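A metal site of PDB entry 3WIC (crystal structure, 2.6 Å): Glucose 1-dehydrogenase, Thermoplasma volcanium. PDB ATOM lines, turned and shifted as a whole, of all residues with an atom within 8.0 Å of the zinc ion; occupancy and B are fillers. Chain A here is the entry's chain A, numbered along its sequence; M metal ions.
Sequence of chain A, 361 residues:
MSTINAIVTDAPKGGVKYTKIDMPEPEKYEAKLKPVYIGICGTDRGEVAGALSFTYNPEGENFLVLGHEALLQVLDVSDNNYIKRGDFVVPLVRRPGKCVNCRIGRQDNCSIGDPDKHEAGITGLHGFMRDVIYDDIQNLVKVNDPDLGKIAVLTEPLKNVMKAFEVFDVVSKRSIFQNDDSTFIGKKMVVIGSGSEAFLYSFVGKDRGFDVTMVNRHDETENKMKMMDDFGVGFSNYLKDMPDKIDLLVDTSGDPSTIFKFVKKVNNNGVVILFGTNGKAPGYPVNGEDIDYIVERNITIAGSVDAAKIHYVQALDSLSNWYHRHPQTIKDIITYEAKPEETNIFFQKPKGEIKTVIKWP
The side-chain amino group (NZ) of Lys 159 lies within salt-bridge range of the side-chain carboxylate (OE1) of Glu 156 (2.9 Å).
N of Thr 43 sits close to SG of Cys 41 (3.4 Å).
The side-chain carboxylate (OE1) of Glu 69 lies within salt-bridge range of the side-chain amino group (NZ) of Lys 355 (3.1 Å).
O of Glu 69 lies within hydrogen-bond range of N of Gly 39 (2.7 Å).
N of Cys 41 is in hydrogen-bond range of OD2 of Asp 44, 2.7 Å away.
Residues that only touch the zinc ion: Glu 156.
Four residues have an atom within 4 Å of the zinc ion: Cys 41, His 68, Glu 69 and Glu 156.
The nearest printed residue that does not touch the zinc ion is Asp 44 (4.2 Å).
The zinc ion is bound by the side-chain carboxylate (OE2) of Glu 69 (2.0 Å).
The zinc ion is bound by NE2 of His 68 (2.2 Å).
The zinc ion is bound by the side-chain sulfur (SG) of Cys 41 (2.3 Å).
The zinc ion has three donor atoms within binding distance.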
ATOM      1  N   GLY A  39      31.928  30.353  25.991  1.00  0.00           N
ATOM      2  CA  GLY A  39      31.733  29.173  25.152  1.00  0.00           C
ATOM      3  C   GLY A  39      30.514  29.316  24.251  1.00  0.00           C
ATOM      4  O   GLY A  39      29.697  30.238  24.441  1.00  0.00           O
ATOM      5  N   ILE A  40      30.366  28.412  23.282  1.00  0.00           N
ATOM      6  CA  ILE A  40      29.229  28.466  22.354  1.00  0.00           C
ATOM      7  C   ILE A  40      28.681  27.086  22.095  1.00  0.00           C
ATOM      8  O   ILE A  40      29.406  26.117  22.155  1.00  0.00           O
ATOM      9  CB  ILE A  40      29.574  29.128  20.998  1.00  0.00           C
ATOM     10  CG1 ILE A  40      30.497  28.223  20.186  1.00  0.00           C
ATOM     11  CG2 ILE A  40      30.169  30.535  21.188  1.00  0.00           C
ATOM     12  CD1 ILE A  40      30.605  28.645  18.726  1.00  0.00           C
ATOM     13  N   CYS A  41      27.389  27.002  21.782  1.00  0.00           N
ATOM     14  CA  CYS A  41      26.772  25.685  21.497  1.00  0.00           C
ATOM     15  C   CYS A  41      25.701  25.840  20.441  1.00  0.00           C
ATOM     16  O   CYS A  41      25.521  26.902  19.887  1.00  0.00           O
ATOM     17  CB  CYS A  41      26.162  25.060  22.793  1.00  0.00           C
ATOM     18  SG  CYS A  41      24.699  25.899  23.464  1.00  0.00           S
ATOM     19  N   GLY A  42      24.982  24.753  20.195  1.00  0.00           N
ATOM     20  CA  GLY A  42      23.890  24.751  19.251  1.00  0.00           C
ATOM     21  C   GLY A  42      22.896  25.871  19.450  1.00  0.00           C
ATOM     22  O   GLY A  42      22.175  26.253  18.533  1.00  0.00           O
ATOM     23  N   THR A  43      22.817  26.384  20.648  1.00  0.00           N
ATOM     24  CA  THR A  43      21.906  27.459  20.898  1.00  0.00           C
ATOM     25  C   THR A  43      22.402  28.729  20.214  1.00  0.00           C
ATOM     26  O   THR A  43      21.605  29.476  19.632  1.00  0.00           O
ATOM     27  CB  THR A  43      21.697  27.672  22.442  1.00  0.00           C
ATOM     28  OG1 THR A  43      21.014  26.538  22.961  1.00  0.00           O
ATOM     29  CG2 THR A  43      20.883  28.932  22.741  1.00  0.00           C
ATOM     30  N   ASP A  44      23.699  28.986  20.342  1.00  0.00           N
ATOM     31  CA  ASP A  44      24.324  30.182  19.795  1.00  0.00           C
ATOM     32  C   ASP A  44      24.125  30.167  18.270  1.00  0.00           C
ATOM     33  O   ASP A  44      23.614  31.126  17.698  1.00  0.00           O
ATOM     34  CB  ASP A  44      25.805  30.237  20.117  1.00  0.00           C
ATOM     35  CG  ASP A  44      26.076  30.504  21.579  1.00  0.00           C
ATOM     36  OD1 ASP A  44      25.970  31.686  21.986  1.00  0.00           O
ATOM     37  OD2 ASP A  44      26.426  29.522  22.288  1.00  0.00           O
ATOM     38  N   GLU A  47      20.657  30.776  17.303  1.00  0.00           N
ATOM     39  CA  GLU A  47      20.172  32.167  17.361  1.00  0.00           C
ATOM     40  C   GLU A  47      20.621  32.908  16.102  1.00  0.00           C
ATOM     41  O   GLU A  47      19.830  33.578  15.419  1.00  0.00           O
ATOM     42  CB  GLU A  47      20.695  32.929  18.580  1.00  0.00           C
ATOM     43  CG  GLU A  47      20.147  32.512  19.953  1.00  0.00           C
ATOM     44  CD  GLU A  47      20.929  33.137  21.128  1.00  0.00           C
ATOM     45  OE1 GLU A  47      20.637  34.267  21.521  1.00  0.00           O
ATOM     46  OE2 GLU A  47      21.859  32.514  21.644  1.00  0.00           O
ATOM     47  N   GLY A  67      25.946  35.321  23.920  1.00  0.00           N
ATOM     48  CA  GLY A  67      26.873  34.622  24.783  1.00  0.00           C
ATOM     49  C   GLY A  67      26.282  34.341  26.142  1.00  0.00           C
ATOM     50  O   GLY A  67      25.949  35.257  26.899  1.00  0.00           O
ATOM     51  N   HIS A  68      26.165  33.061  26.465  1.00  0.00           N
ATOM     52  CA  HIS A  68      25.529  32.697  27.721  1.00  0.00           C
ATOM     53  C   HIS A  68      26.436  31.825  28.612  1.00  0.00           C
ATOM     54  O   HIS A  68      26.177  31.767  29.794  1.00  0.00           O
ATOM     55  CB  HIS A  68      24.175  32.019  27.491  1.00  0.00           C
ATOM     56  CG  HIS A  68      24.235  30.872  26.554  1.00  0.00           C
ATOM     57  ND1 HIS A  68      24.446  31.037  25.205  1.00  0.00           N
ATOM     58  CD2 HIS A  68      24.145  29.541  26.767  1.00  0.00           C
ATOM     59  CE1 HIS A  68      24.485  29.852  24.618  1.00  0.00           C
ATOM     60  NE2 HIS A  68      24.305  28.930  25.536  1.00  0.00           N
ATOM     61  N   GLU A  69      27.491  31.213  28.042  1.00  0.00           N
ATOM     62  CA  GLU A  69      28.443  30.372  28.735  1.00  0.00           C
ATOM     63  C   GLU A  69      29.732  31.157  29.052  1.00  0.00           C
ATOM     64  O   GLU A  69      30.686  31.092  28.300  1.00  0.00           O
ATOM     65  CB  GLU A  69      28.827  29.214  27.824  1.00  0.00           C
ATOM     66  CG  GLU A  69      27.641  28.504  27.141  1.00  0.00           C
ATOM     67  CD  GLU A  69      28.114  27.329  26.348  1.00  0.00           C
ATOM     68  OE1 GLU A  69      29.329  27.108  26.373  1.00  0.00           O
ATOM     69  OE2 GLU A  69      27.305  26.654  25.685  1.00  0.00           O
ATOM     70  N   VAL A  93      22.789  32.578  33.917  1.00  0.00           N
ATOM     71  CA  VAL A  93      22.139  32.831  32.654  1.00  0.00           C
ATOM     72  C   VAL A  93      20.714  33.235  32.847  1.00  0.00           C
ATOM     73  O   VAL A  93      20.267  34.273  32.361  1.00  0.00           O
ATOM     74  CB  VAL A  93      22.122  31.600  31.712  1.00  0.00           C
ATOM     75  CG1 VAL A  93      21.456  32.008  30.386  1.00  0.00           C
ATOM     76  CG2 VAL A  93      23.522  31.068  31.446  1.00  0.00           C
ATOM     77  N   ILE A 122      19.838  35.386  25.325  1.00  0.00           N
ATOM     78  CA  ILE A 122      18.764  34.699  24.641  1.00  0.00           C
ATOM     79  C   ILE A 122      17.420  35.440  24.587  1.00  0.00           C
ATOM     80  O   ILE A 122      16.845  35.623  23.541  1.00  0.00           O
ATOM     81  CB  ILE A 122      18.657  33.273  25.179  1.00  0.00           C
ATOM     82  CG1 ILE A 122      20.053  32.667  25.274  1.00  0.00           C
ATOM     83  CG2 ILE A 122      17.842  32.444  24.242  1.00  0.00           C
ATOM     84  CD1 ILE A 122      20.248  31.431  26.120  1.00  0.00           C
ATOM     85  N   GLU A 156      28.614  26.513  32.494  1.00  0.00           N
ATOM     86  CA  GLU A 156      27.232  26.749  32.063  1.00  0.00           C
ATOM     87  C   GLU A 156      26.688  25.515  31.408  1.00  0.00           C
ATOM     88  O   GLU A 156      25.581  25.141  31.687  1.00  0.00           O
ATOM     89  CB  GLU A 156      27.120  27.971  31.132  1.00  0.00           C
ATOM     90  CG  GLU A 156      25.712  28.539  30.951  1.00  0.00           C
ATOM     91  CD  GLU A 156      24.878  27.767  29.969  1.00  0.00           C
ATOM     92  OE1 GLU A 156      23.633  27.890  30.023  1.00  0.00           O
ATOM     93  OE2 GLU A 156      25.467  27.007  29.149  1.00  0.00           O
ATOM     94  N   PRO A 157      27.452  24.854  30.551  1.00  0.00           N
ATOM     95  CA  PRO A 157      26.854  23.623  29.973  1.00  0.00           C
ATOM     96  C   PRO A 157      26.628  22.504  30.977  1.00  0.00           C
ATOM     97  O   PRO A 157      25.681  21.748  30.857  1.00  0.00           O
ATOM     98  CB  PRO A 157      27.887  23.178  28.924  1.00  0.00           C
ATOM     99  CG  PRO A 157      28.709  24.397  28.649  1.00  0.00           C
ATOM    100  CD  PRO A 157      28.736  25.181  29.929  1.00  0.00           C
ATOM    101  N   LYS A 159      26.040  22.603  34.311  1.00  0.00           N
ATOM    102  CA  LYS A 159      24.963  22.860  35.234  1.00  0.00           C
ATOM    103  C   LYS A 159      23.600  22.430  34.726  1.00  0.00           C
ATOM    104  O   LYS A 159      22.738  22.147  35.527  1.00  0.00           O
ATOM    105  CB  LYS A 159      24.942  24.316  35.703  1.00  0.00           C
ATOM    106  CG  LYS A 159      24.778  25.381  34.655  1.00  0.00           C
ATOM    107  CD  LYS A 159      23.363  25.575  34.112  1.00  0.00           C
ATOM    108  CE  LYS A 159      23.414  26.662  33.081  1.00  0.00           C
ATOM    109  NZ  LYS A 159      22.192  26.863  32.329  1.00  0.00           N
ATOM    110  N   ASN A 160      23.390  22.401  33.422  1.00  0.00           N
ATOM    111  CA  ASN A 160      22.183  21.797  32.873  1.00  0.00           C
ATOM    112  C   ASN A 160      22.076  20.327  33.114  1.00  0.00           C
ATOM    113  O   ASN A 160      20.983  19.808  33.319  1.00  0.00           O
ATOM    114  CB  ASN A 160      22.123  22.011  31.376  1.00  0.00           C
ATOM    115  CG  ASN A 160      21.965  23.449  31.016  1.00  0.00           C
ATOM    116  OD1 ASN A 160      21.283  24.196  31.710  1.00  0.00           O
ATOM    117  ND2 ASN A 160      22.587  23.863  29.903  1.00  0.00           N
ATOM    118  N   SER A 196      29.457  17.846  23.183  1.00  0.00           N
ATOM    119  CA  SER A 196      29.918  18.292  24.505  1.00  0.00           C
ATOM    120  C   SER A 196      28.873  17.926  25.572  1.00  0.00           C
ATOM    121  O   SER A 196      29.192  17.304  26.563  1.00  0.00           O
ATOM    122  CB  SER A 196      30.178  19.784  24.489  1.00  0.00           C
ATOM    123  OG  SER A 196      29.011  20.434  24.014  1.00  0.00           O
ATOM    124  N   GLU A 197      27.615  18.250  25.329  1.00  0.00           N
ATOM    125  CA  GLU A 197      26.568  17.882  26.274  1.00  0.00           C
ATOM    126  C   GLU A 197      26.548  16.376  26.608  1.00  0.00           C
ATOM    127  O   GLU A 197      26.565  16.007  27.748  1.00  0.00           O
ATOM    128  CB  GLU A 197      25.202  18.309  25.754  1.00  0.00           C
ATOM    129  CG  GLU A 197      25.076  19.799  25.598  1.00  0.00           C
ATOM    130  CD  GLU A 197      25.259  20.278  24.149  1.00  0.00           C
ATOM    131  OE1 GLU A 197      24.648  21.323  23.845  1.00  0.00           O
ATOM    132  OE2 GLU A 197      25.979  19.642  23.335  1.00  0.00           O
ATOM    133  N   LYS A 355      34.030  21.444  22.117  1.00  0.00           N
ATOM    134  CA  LYS A 355      33.660  22.752  22.622  1.00  0.00           C
ATOM    135  C   LYS A 355      34.494  23.854  22.014  1.00  0.00           C
ATOM    136  O   LYS A 355      35.708  23.869  22.067  1.00  0.00           O
ATOM    137  CB  LYS A 355      33.795  22.719  24.141  1.00  0.00           C
ATOM    138  CG  LYS A 355      33.606  24.019  24.874  1.00  0.00           C
ATOM    139  CD  LYS A 355      32.295  24.651  24.490  1.00  0.00           C
ATOM    140  CE  LYS A 355      31.149  24.156  25.318  1.00  0.00           C
ATOM    141  NZ  LYS A 355      29.911  24.591  24.653  1.00  0.00           N
HETATM  142 ZN    ZN M   1      25.320  26.950  25.442  1.00  0.00          ZN
